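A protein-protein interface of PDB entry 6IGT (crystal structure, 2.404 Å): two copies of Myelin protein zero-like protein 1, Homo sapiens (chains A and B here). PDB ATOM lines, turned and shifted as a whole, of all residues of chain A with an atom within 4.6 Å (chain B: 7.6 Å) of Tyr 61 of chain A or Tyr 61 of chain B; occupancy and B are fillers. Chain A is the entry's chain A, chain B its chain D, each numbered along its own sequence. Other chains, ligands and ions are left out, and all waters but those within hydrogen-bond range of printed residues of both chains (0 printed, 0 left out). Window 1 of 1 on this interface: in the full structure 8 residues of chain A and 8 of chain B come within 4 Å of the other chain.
ND1 of His 54 of chain A sits at hydrogen-bond distance from OG of Ser 38 of chain A (2.8 Å).
O of Phe 52 of chain A is in hydrogen-bond range of N of Gly 63 of chain A.
The backbone NH of Tyr 61 of chain A lies within hydrogen-bond range of the backbone carbonyl oxygen of His 54 of chain A (2.9 Å).
A ring nitrogen (ND1) of His 54 of chain B is in hydrogen-bond range of the side-chain hydroxyl of Ser 38 of chain B, at 2.7 Å.
The backbone NH of Trp 39 of chain B is in hydrogen-bond range of the backbone carbonyl oxygen of Phe 53 of chain B.
A ring nitrogen (NE2) of His 54 of chain B is in hydrogen-bond range of the side-chain hydroxyl of Ser 56 of chain B.
Printed residues of chain B within 4 Å of Phe 53 of chain A: Tyr 61 (3.7 Å).
Of the printed residues of chain B, Val 60 of chain A touches Gly 63.
Of the printed residues of chain A, His 54 of chain B touches His 54 (3.2 Å) and Tyr 61 (3.8 Å).
Of the printed residues of chain A, Gln 59 of chain B touches Ser 51 (3.3 Å) and Gly 63 (3.9 Å).
Of the printed residues of chain A, Gly 63 of chain B touches Gln 59 (3.9998 Å) and Val 60 (3.7 Å).
The nearest printed residue of chain B that does not touch Tyr 61 of chain A is Gly 63 of chain B (4.01 Å).
His 54 of chain B touches its own counterpart, His 54 of chain A.
Gln 59 of chain A touches Gly 63 of chain B, and with the chains exchanged Gly 63 of chain A touches Gln 59 of chain B.
Val 60 of chain A touches Gly 63 of chain B, and with the chains exchanged Gly 63 of chain A touches Val 60 of chain B.
Tyr 61 of chain A touches Leu 62 of chain B, and with the chains exchanged Leu 62 of chain A touches Tyr 61 of chain B.
Of the 17 pairs that touch across the chains among the printed residues, 17 have their exchanged pair printed and touching as well.
OE1 of Gln 59 of chain B sits close to O of Ser 51 of chain A (3.3 Å).
The side-chain hydroxyl of Tyr 61 of chain B is in hydrogen-bond range of the side-chain hydroxyl of Ser 51 of chain A, 2.6 Å away.
NE2 of His 54 of chain B sits at hydrogen-bond distance from NE2 of His 54 of chain A (3.2 Å).
The side-chain amide oxygen (OE1) of Gln 59 of chain A lies close to the backbone carbonyl oxygen (O) of Ser 51 of chain B (3.3 Å).
OH of Tyr 61 of chain A is in hydrogen-bond range of OG of Ser 51 of chain B (2.5 Å).
The backbone NH (N) of Leu 62 of chain A sits at hydrogen-bond distance from the backbone carbonyl oxygen (O) of Leu 62 of chain B (2.8 Å).
Among the printed residues, merely in contact across the chains: Phe 53 of chain A with Tyr 61 of chain B (3.7 Å), His 54 of chain A with Tyr 61 of chain B (3.8 Å), Gln 59 of chain A with Gly 63 of chain B (3.9998 Å), Val 60 of chain A with Gly 63 of chain B (3.7 Å), Tyr 61 of chain A with Phe 53 of chain B (3.6 Å), Tyr 61 of chain A with His 54 of chain B (3.8 Å), Tyr 61 of chain A with Tyr 61 of chain B (3.4 Å), Tyr 61 of chain A with Leu 62 of chain B (3.3 Å), Leu 62 of chain A with Tyr 61 of chain B (3.2 Å), Gly 63 of chain A with Gln 59 of chain B (3.9 Å) and Gly 63 of chain A with Val 60 of chain B (3.8 Å).
Hydrophobic or aromatic side chains of chain B that line the printed part of chain A: His 54 and Tyr 61.
Hydrophobic or aromatic side chains of chain A within 4 Å of the printed part of chain B: His 54 and Tyr 61.
Among the printed residues, no Asp or Glu carboxylate lies within 4 Å of a Lys or Arg side-chain nitrogen of the other chain.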
ATOM      1  N   SER A  38      -7.028   3.249  10.117  1.00  0.00           N
ATOM      2  CA  SER A  38      -7.957   2.165  10.413  1.00  0.00           C
ATOM      3  C   SER A  38      -9.308   2.746  10.842  1.00  0.00           C
ATOM      4  O   SER A  38      -9.367   3.764  11.534  1.00  0.00           O
ATOM      5  CB  SER A  38      -7.404   1.266  11.504  1.00  0.00           C
ATOM      6  OG  SER A  38      -6.279   0.559  11.030  1.00  0.00           O
ATOM      7  N   SER A  51     -13.254  -3.747  13.724  1.00  0.00           N
ATOM      8  CA  SER A  51     -12.388  -3.021  12.815  1.00  0.00           C
ATOM      9  C   SER A  51     -12.586  -3.575  11.406  1.00  0.00           C
ATOM     10  O   SER A  51     -12.450  -4.787  11.191  1.00  0.00           O
ATOM     11  CB  SER A  51     -10.940  -3.151  13.274  1.00  0.00           C
ATOM     12  OG  SER A  51     -10.159  -2.104  12.729  1.00  0.00           O
ATOM     13  N   PHE A  52     -12.916  -2.690  10.444  1.00  0.00           N
ATOM     14  CA  PHE A  52     -13.349  -3.140   9.115  1.00  0.00           C
ATOM     15  C   PHE A  52     -12.599  -2.546   7.927  1.00  0.00           C
ATOM     16  O   PHE A  52     -12.851  -2.974   6.796  1.00  0.00           O
ATOM     17  CB  PHE A  52     -14.856  -2.872   8.908  1.00  0.00           C
ATOM     18  CG  PHE A  52     -15.239  -1.424   8.893  1.00  0.00           C
ATOM     19  CD1 PHE A  52     -15.496  -0.758  10.072  1.00  0.00           C
ATOM     20  CD2 PHE A  52     -15.379  -0.734   7.701  1.00  0.00           C
ATOM     21  CE1 PHE A  52     -15.867   0.577  10.074  1.00  0.00           C
ATOM     22  CE2 PHE A  52     -15.747   0.611   7.692  1.00  0.00           C
ATOM     23  CZ  PHE A  52     -16.007   1.265   8.890  1.00  0.00           C
ATOM     24  N   PHE A  53     -11.697  -1.595   8.131  1.00  0.00           N
ATOM     25  CA  PHE A  53     -11.011  -0.954   7.021  1.00  0.00           C
ATOM     26  C   PHE A  53      -9.608  -0.599   7.472  1.00  0.00           C
ATOM     27  O   PHE A  53      -9.398  -0.198   8.619  1.00  0.00           O
ATOM     28  CB  PHE A  53     -11.779   0.292   6.560  1.00  0.00           C
ATOM     29  CG  PHE A  53     -11.030   1.170   5.585  1.00  0.00           C
ATOM     30  CD1 PHE A  53     -11.324   1.127   4.240  1.00  0.00           C
ATOM     31  CD2 PHE A  53     -10.081   2.079   6.021  1.00  0.00           C
ATOM     32  CE1 PHE A  53     -10.666   1.945   3.353  1.00  0.00           C
ATOM     33  CE2 PHE A  53      -9.415   2.892   5.131  1.00  0.00           C
ATOM     34  CZ  PHE A  53      -9.712   2.828   3.807  1.00  0.00           C
ATOM     35  N   HIS A  54      -8.654  -0.741   6.565  1.00  0.00           N
ATOM     36  CA  HIS A  54      -7.281  -0.361   6.857  1.00  0.00           C
ATOM     37  C   HIS A  54      -6.625   0.132   5.582  1.00  0.00           C
ATOM     38  O   HIS A  54      -6.827  -0.441   4.513  1.00  0.00           O
ATOM     39  CB  HIS A  54      -6.472  -1.515   7.441  1.00  0.00           C
ATOM     40  CG  HIS A  54      -5.063  -1.142   7.786  1.00  0.00           C
ATOM     41  ND1 HIS A  54      -4.740  -0.434   8.922  1.00  0.00           N
ATOM     42  CD2 HIS A  54      -3.898  -1.361   7.135  1.00  0.00           C
ATOM     43  CE1 HIS A  54      -3.434  -0.242   8.962  1.00  0.00           C
ATOM     44  NE2 HIS A  54      -2.901  -0.793   7.888  1.00  0.00           N
ATOM     45  N   SER A  56      -2.817   1.528   4.163  1.00  0.00           N
ATOM     46  CA  SER A  56      -1.405   1.868   4.275  1.00  0.00           C
ATOM     47  C   SER A  56      -0.696   1.440   3.003  1.00  0.00           C
ATOM     48  O   SER A  56      -1.098   0.472   2.347  1.00  0.00           O
ATOM     49  CB  SER A  56      -0.750   1.233   5.497  1.00  0.00           C
ATOM     50  OG  SER A  56      -1.034  -0.153   5.579  1.00  0.00           O
ATOM     51  N   GLN A  59      -2.594   1.089  -0.264  1.00  0.00           N
ATOM     52  CA  GLN A  59      -3.423  -0.105  -0.415  1.00  0.00           C
ATOM     53  C   GLN A  59      -4.622  -0.064   0.528  1.00  0.00           C
ATOM     54  O   GLN A  59      -4.484   0.265   1.709  1.00  0.00           O
ATOM     55  CB  GLN A  59      -2.600  -1.375  -0.175  1.00  0.00           C
ATOM     56  CG  GLN A  59      -3.414  -2.655  -0.247  1.00  0.00           C
ATOM     57  CD  GLN A  59      -4.048  -2.865  -1.607  1.00  0.00           C
ATOM     58  OE1 GLN A  59      -3.368  -2.842  -2.617  1.00  0.00           O
ATOM     59  NE2 GLN A  59      -5.356  -3.081  -1.636  1.00  0.00           N
ATOM     60  N   VAL A  60      -5.789  -0.404   0.005  1.00  0.00           N
ATOM     61  CA  VAL A  60      -6.999  -0.555   0.800  1.00  0.00           C
ATOM     62  C   VAL A  60      -7.181  -2.028   1.127  1.00  0.00           C
ATOM     63  O   VAL A  60      -7.189  -2.871   0.220  1.00  0.00           O
ATOM     64  CB  VAL A  60      -8.230  -0.027   0.047  1.00  0.00           C
ATOM     65  CG1 VAL A  60      -9.480  -0.383   0.803  1.00  0.00           C
ATOM     66  CG2 VAL A  60      -8.126   1.466  -0.162  1.00  0.00           C
ATOM     67  N   TYR A  61      -7.340  -2.337   2.416  1.00  0.00           N
ATOM     68  CA  TYR A  61      -7.678  -3.676   2.892  1.00  0.00           C
ATOM     69  C   TYR A  61      -8.994  -3.622   3.660  1.00  0.00           C
ATOM     70  O   TYR A  61      -9.215  -2.698   4.453  1.00  0.00           O
ATOM     71  CB  TYR A  61      -6.614  -4.238   3.832  1.00  0.00           C
ATOM     72  CG  TYR A  61      -5.166  -4.079   3.442  1.00  0.00           C
ATOM     73  CD1 TYR A  61      -4.437  -5.159   2.948  1.00  0.00           C
ATOM     74  CD2 TYR A  61      -4.499  -2.875   3.645  1.00  0.00           C
ATOM     75  CE1 TYR A  61      -3.109  -5.029   2.632  1.00  0.00           C
ATOM     76  CE2 TYR A  61      -3.175  -2.739   3.326  1.00  0.00           C
ATOM     77  CZ  TYR A  61      -2.483  -3.819   2.814  1.00  0.00           C
ATOM     78  OH  TYR A  61      -1.149  -3.678   2.500  1.00  0.00           O
ATOM     79  N   LEU A  62      -9.847  -4.633   3.475  1.00  0.00           N
ATOM     80  CA  LEU A  62     -11.159  -4.673   4.115  1.00  0.00           C
ATOM     81  C   LEU A  62     -11.291  -5.874   5.045  1.00  0.00           C
ATOM     82  O   LEU A  62     -10.700  -6.933   4.814  1.00  0.00           O
ATOM     83  CB  LEU A  62     -12.285  -4.709   3.077  1.00  0.00           C
ATOM     84  CG  LEU A  62     -12.309  -3.527   2.112  1.00  0.00           C
ATOM     85  CD1 LEU A  62     -13.403  -3.713   1.067  1.00  0.00           C
ATOM     86  CD2 LEU A  62     -12.470  -2.184   2.841  1.00  0.00           C
ATOM     87  N   GLY A  63     -12.063  -5.687   6.127  1.00  0.00           N
ATOM     88  CA  GLY A  63     -12.466  -6.791   6.983  1.00  0.00           C
ATOM     89  C   GLY A  63     -13.649  -7.523   6.391  1.00  0.00           C
ATOM     90  O   GLY A  63     -14.185  -7.112   5.375  1.00  0.00           O
ATOM     91  N   VAL B  37       1.285  -7.212  10.623  1.00  0.00           N
ATOM     92  CA  VAL B  37       1.798  -8.036   9.535  1.00  0.00           C
ATOM     93  C   VAL B  37       1.136  -7.610   8.237  1.00  0.00           C
ATOM     94  O   VAL B  37      -0.075  -7.372   8.201  1.00  0.00           O
ATOM     95  CB  VAL B  37       1.538  -9.526   9.788  1.00  0.00           C
ATOM     96  CG1 VAL B  37       2.082 -10.355   8.635  1.00  0.00           C
ATOM     97  CG2 VAL B  37       2.171  -9.942  11.106  1.00  0.00           C
ATOM     98  N   SER B  38       1.927  -7.532   7.178  1.00  0.00           N
ATOM     99  CA  SER B  38       1.446  -7.351   5.818  1.00  0.00           C
ATOM    100  C   SER B  38       2.142  -8.358   4.909  1.00  0.00           C
ATOM    101  O   SER B  38       3.340  -8.612   5.060  1.00  0.00           O
ATOM    102  CB  SER B  38       1.705  -5.938   5.345  1.00  0.00           C
ATOM    103  OG  SER B  38       0.942  -5.016   6.105  1.00  0.00           O
ATOM    104  N   TRP B  39       1.391  -8.951   3.985  1.00  0.00           N
ATOM    105  CA  TRP B  39       1.949  -9.853   2.988  1.00  0.00           C
ATOM    106  C   TRP B  39       1.737  -9.257   1.606  1.00  0.00           C
ATOM    107  O   TRP B  39       0.670  -8.704   1.319  1.00  0.00           O
ATOM    108  CB  TRP B  39       1.306 -11.239   3.039  1.00  0.00           C
ATOM    109  CG  TRP B  39       1.863 -12.168   4.063  1.00  0.00           C
ATOM    110  CD1 TRP B  39       1.407 -12.353   5.336  1.00  0.00           C
ATOM    111  CD2 TRP B  39       2.964 -13.067   3.895  1.00  0.00           C
ATOM    112  NE1 TRP B  39       2.161 -13.297   5.970  1.00  0.00           N
ATOM    113  CE2 TRP B  39       3.124 -13.755   5.112  1.00  0.00           C
ATOM    114  CE3 TRP B  39       3.831 -13.359   2.830  1.00  0.00           C
ATOM    115  CZ2 TRP B  39       4.128 -14.720   5.305  1.00  0.00           C
ATOM    116  CZ3 TRP B  39       4.827 -14.309   3.018  1.00  0.00           C
ATOM    117  CH2 TRP B  39       4.963 -14.987   4.243  1.00  0.00           C
ATOM    118  N   SER B  40       2.743  -9.408   0.748  1.00  0.00           N
ATOM    119  CA  SER B  40       2.713  -8.889  -0.605  1.00  0.00           C
ATOM    120  C   SER B  40       3.071  -9.977  -1.610  1.00  0.00           C
ATOM    121  O   SER B  40       3.742 -10.957  -1.289  1.00  0.00           O
ATOM    122  CB  SER B  40       3.665  -7.717  -0.735  1.00  0.00           C
ATOM    123  OG  SER B  40       3.229  -6.720   0.151  1.00  0.00           O
ATOM    124  N   VAL B  50       1.778  -6.486  -5.370  1.00  0.00           N
ATOM    125  CA  VAL B  50       0.472  -6.222  -4.773  1.00  0.00           C
ATOM    126  C   VAL B  50       0.528  -6.615  -3.309  1.00  0.00           C
ATOM    127  O   VAL B  50       0.758  -7.791  -2.985  1.00  0.00           O
ATOM    128  CB  VAL B  50      -0.650  -7.034  -5.444  1.00  0.00           C
ATOM    129  CG1 VAL B  50      -1.965  -6.282  -5.376  1.00  0.00           C
ATOM    130  CG2 VAL B  50      -0.296  -7.459  -6.830  1.00  0.00           C
ATOM    131  N   SER B  51       0.253  -5.667  -2.430  1.00  0.00           N
ATOM    132  CA  SER B  51       0.019  -5.967  -1.029  1.00  0.00           C
ATOM    133  C   SER B  51      -1.431  -6.423  -0.871  1.00  0.00           C
ATOM    134  O   SER B  51      -2.355  -5.679  -1.225  1.00  0.00           O
ATOM    135  CB  SER B  51       0.310  -4.743  -0.170  1.00  0.00           C
ATOM    136  OG  SER B  51       0.366  -5.113   1.206  1.00  0.00           O
ATOM    137  N   PHE B  52      -1.629  -7.646  -0.344  1.00  0.00           N
ATOM    138  CA  PHE B  52      -2.948  -8.277  -0.333  1.00  0.00           C
ATOM    139  C   PHE B  52      -3.467  -8.703   1.037  1.00  0.00           C
ATOM    140  O   PHE B  52      -4.622  -9.140   1.130  1.00  0.00           O
ATOM    141  CB  PHE B  52      -2.969  -9.510  -1.263  1.00  0.00           C
ATOM    142  CG  PHE B  52      -2.083 -10.629  -0.823  1.00  0.00           C
ATOM    143  CD1 PHE B  52      -0.750 -10.654  -1.194  1.00  0.00           C
ATOM    144  CD2 PHE B  52      -2.579 -11.668  -0.045  1.00  0.00           C
ATOM    145  CE1 PHE B  52       0.087 -11.682  -0.787  1.00  0.00           C
ATOM    146  CE2 PHE B  52      -1.751 -12.712   0.369  1.00  0.00           C
ATOM    147  CZ  PHE B  52      -0.415 -12.722  -0.020  1.00  0.00           C
ATOM    148  N   PHE B  53      -2.685  -8.580   2.096  1.00  0.00           N
ATOM    149  CA  PHE B  53      -3.131  -9.070   3.391  1.00  0.00           C
ATOM    150  C   PHE B  53      -2.536  -8.194   4.474  1.00  0.00           C
ATOM    151  O   PHE B  53      -1.362  -7.830   4.410  1.00  0.00           O
ATOM    152  CB  PHE B  53      -2.718 -10.533   3.588  1.00  0.00           C
ATOM    153  CG  PHE B  53      -2.888 -11.037   4.989  1.00  0.00           C
ATOM    154  CD1 PHE B  53      -3.952 -11.861   5.311  1.00  0.00           C
ATOM    155  CD2 PHE B  53      -1.967 -10.723   5.986  1.00  0.00           C
ATOM    156  CE1 PHE B  53      -4.100 -12.342   6.595  1.00  0.00           C
ATOM    157  CE2 PHE B  53      -2.124 -11.199   7.263  1.00  0.00           C
ATOM    158  CZ  PHE B  53      -3.182 -12.007   7.564  1.00  0.00           C
ATOM    159  N   HIS B  54      -3.341  -7.888   5.479  1.00  0.00           N
ATOM    160  CA  HIS B  54      -2.861  -7.123   6.618  1.00  0.00           C
ATOM    161  C   HIS B  54      -3.504  -7.647   7.890  1.00  0.00           C
ATOM    162  O   HIS B  54      -4.690  -7.977   7.897  1.00  0.00           O
ATOM    163  CB  HIS B  54      -3.163  -5.644   6.462  1.00  0.00           C
ATOM    164  CG  HIS B  54      -2.601  -4.806   7.567  1.00  0.00           C
ATOM    165  ND1 HIS B  54      -1.256  -4.531   7.680  1.00  0.00           N
ATOM    166  CD2 HIS B  54      -3.199  -4.198   8.617  1.00  0.00           C
ATOM    167  CE1 HIS B  54      -1.053  -3.781   8.747  1.00  0.00           C
ATOM    168  NE2 HIS B  54      -2.215  -3.561   9.328  1.00  0.00           N
ATOM    169  N   TYR B  55      -2.712  -7.726   8.960  1.00  0.00           N
ATOM    170  CA  TYR B  55      -3.171  -8.204  10.261  1.00  0.00           C
ATOM    171  C   TYR B  55      -2.686  -7.279  11.362  1.00  0.00           C
ATOM    172  O   TYR B  55      -1.477  -7.162  11.581  1.00  0.00           O
ATOM    173  CB  TYR B  55      -2.665  -9.617  10.553  1.00  0.00           C
ATOM    174  CG  TYR B  55      -3.264 -10.208  11.816  1.00  0.00           C
ATOM    175  CD1 TYR B  55      -2.682  -9.992  13.068  1.00  0.00           C
ATOM    176  CD2 TYR B  55      -4.435 -10.969  11.757  1.00  0.00           C
ATOM    177  CE1 TYR B  55      -3.239 -10.540  14.215  1.00  0.00           C
ATOM    178  CE2 TYR B  55      -4.997 -11.511  12.891  1.00  0.00           C
ATOM    179  CZ  TYR B  55      -4.397 -11.299  14.114  1.00  0.00           C
ATOM    180  OH  TYR B  55      -4.985 -11.854  15.219  1.00  0.00           O
ATOM    181  N   SER B  56      -3.618  -6.661  12.080  1.00  0.00           N
ATOM    182  CA  SER B  56      -3.257  -5.943  13.297  1.00  0.00           C
ATOM    183  C   SER B  56      -4.469  -5.858  14.205  1.00  0.00           C
ATOM    184  O   SER B  56      -5.587  -5.635  13.737  1.00  0.00           O
ATOM    185  CB  SER B  56      -2.710  -4.543  13.014  1.00  0.00           C
ATOM    186  OG  SER B  56      -3.599  -3.800  12.206  1.00  0.00           O
ATOM    187  N   GLN B  57      -4.228  -6.077  15.503  1.00  0.00           N
ATOM    188  CA  GLN B  57      -5.242  -5.980  16.555  1.00  0.00           C
ATOM    189  C   GLN B  57      -6.328  -7.043  16.401  1.00  0.00           C
ATOM    190  O   GLN B  57      -7.523  -6.748  16.431  1.00  0.00           O
ATOM    191  CB  GLN B  57      -5.845  -4.582  16.604  1.00  0.00           C
ATOM    192  CG  GLN B  57      -5.264  -3.775  17.730  1.00  0.00           C
ATOM    193  CD  GLN B  57      -4.967  -2.349  17.329  1.00  0.00           C
ATOM    194  OE1 GLN B  57      -5.381  -1.890  16.257  1.00  0.00           O
ATOM    195  NE2 GLN B  57      -4.239  -1.635  18.191  1.00  0.00           N
ATOM    196  N   GLY B  58      -5.901  -8.289  16.261  1.00  0.00           N
ATOM    197  CA  GLY B  58      -6.854  -9.376  16.138  1.00  0.00           C
ATOM    198  C   GLY B  58      -7.730  -9.331  14.909  1.00  0.00           C
ATOM    199  O   GLY B  58      -8.716 -10.063  14.847  1.00  0.00           O
ATOM    200  N   GLN B  59      -7.409  -8.501  13.917  1.00  0.00           N
ATOM    201  CA  GLN B  59      -8.269  -8.353  12.745  1.00  0.00           C
ATOM    202  C   GLN B  59      -7.502  -8.637  11.458  1.00  0.00           C
ATOM    203  O   GLN B  59      -6.447  -8.043  11.204  1.00  0.00           O
ATOM    204  CB  GLN B  59      -8.886  -6.955  12.690  1.00  0.00           C
ATOM    205  CG  GLN B  59      -9.750  -6.746  11.466  1.00  0.00           C
ATOM    206  CD  GLN B  59     -10.941  -7.668  11.445  1.00  0.00           C
ATOM    207  OE1 GLN B  59     -11.667  -7.756  12.415  1.00  0.00           O
ATOM    208  NE2 GLN B  59     -11.147  -8.362  10.333  1.00  0.00           N
ATOM    209  N   VAL B  60      -8.047  -9.540  10.653  1.00  0.00           N
ATOM    210  CA  VAL B  60      -7.574  -9.800   9.298  1.00  0.00           C
ATOM    211  C   VAL B  60      -8.266  -8.837   8.341  1.00  0.00           C
ATOM    212  O   VAL B  60      -9.499  -8.716   8.359  1.00  0.00           O
ATOM    213  CB  VAL B  60      -7.872 -11.252   8.889  1.00  0.00           C
ATOM    214  CG1 VAL B  60      -7.510 -11.466   7.448  1.00  0.00           C
ATOM    215  CG2 VAL B  60      -7.151 -12.229   9.800  1.00  0.00           C
ATOM    216  N   TYR B  61      -7.476  -8.168   7.495  1.00  0.00           N
ATOM    217  CA  TYR B  61      -7.972  -7.324   6.413  1.00  0.00           C
ATOM    218  C   TYR B  61      -7.378  -7.798   5.092  1.00  0.00           C
ATOM    219  O   TYR B  61      -6.164  -8.009   4.999  1.00  0.00           O
ATOM    220  CB  TYR B  61      -7.598  -5.854   6.606  1.00  0.00           C
ATOM    221  CG  TYR B  61      -7.778  -5.235   7.973  1.00  0.00           C
ATOM    222  CD1 TYR B  61      -8.844  -4.372   8.238  1.00  0.00           C
ATOM    223  CD2 TYR B  61      -6.837  -5.441   8.976  1.00  0.00           C
ATOM    224  CE1 TYR B  61      -8.990  -3.774   9.476  1.00  0.00           C
ATOM    225  CE2 TYR B  61      -6.976  -4.852  10.219  1.00  0.00           C
ATOM    226  CZ  TYR B  61      -8.050  -4.021  10.467  1.00  0.00           C
ATOM    227  OH  TYR B  61      -8.161  -3.433  11.711  1.00  0.00           O
ATOM    228  N   LEU B  62      -8.216  -7.910   4.060  1.00  0.00           N
ATOM    229  CA  LEU B  62      -7.805  -8.419   2.753  1.00  0.00           C
ATOM    230  C   LEU B  62      -7.913  -7.347   1.682  1.00  0.00           C
ATOM    231  O   LEU B  62      -8.827  -6.509   1.713  1.00  0.00           O
ATOM    232  CB  LEU B  62      -8.639  -9.631   2.350  1.00  0.00           C
ATOM    233  CG  LEU B  62      -8.608 -10.818   3.306  1.00  0.00           C
ATOM    234  CD1 LEU B  62      -9.547 -11.864   2.782  1.00  0.00           C
ATOM    235  CD2 LEU B  62      -7.219 -11.404   3.458  1.00  0.00           C
ATOM    236  N   GLY B  63      -6.956  -7.368   0.740  1.00  0.00           N
ATOM    237  CA  GLY B  63      -7.034  -6.505  -0.428  1.00  0.00           C
ATOM    238  C   GLY B  63      -7.869  -7.126  -1.521  1.00  0.00           C
ATOM    239  O   GLY B  63      -8.261  -8.273  -1.416  1.00  0.00           O
ATOM    240  N   ASN B  64      -8.166  -6.374  -2.581  1.00  0.00           N
ATOM    241  CA  ASN B  64      -9.052  -6.899  -3.631  1.00  0.00           C
ATOM    242  C   ASN B  64      -8.279  -7.318  -4.888  1.00  0.00           C
ATOM    243  O   ASN B  64      -8.543  -6.874  -6.003  1.00  0.00           O
ATOM    244  CB  ASN B  64     -10.139  -5.888  -3.969  1.00  0.00           C
ATOM    245  CG  ASN B  64      -9.620  -4.663  -4.683  1.00  0.00           C
ATOM    246  OD1 ASN B  64      -8.413  -4.453  -4.798  1.00  0.00           O
ATOM    247  ND2 ASN B  64     -10.545  -3.837  -5.171  1.00  0.00           N
ATOM    248  N   ILE B  72      -7.388 -16.688   1.007  1.00  0.00           N
ATOM    249  CA  ILE B  72      -6.387 -16.270   1.976  1.00  0.00           C
ATOM    250  C   ILE B  72      -6.952 -16.438   3.375  1.00  0.00           C
ATOM    251  O   ILE B  72      -8.065 -15.985   3.666  1.00  0.00           O
ATOM    252  CB  ILE B  72      -5.962 -14.812   1.737  1.00  0.00           C
ATOM    253  CG1 ILE B  72      -5.443 -14.624   0.320  1.00  0.00           C
ATOM    254  CG2 ILE B  72      -4.934 -14.388   2.786  1.00  0.00           C
ATOM    255  CD1 ILE B  72      -4.319 -15.552  -0.032  1.00  0.00           C
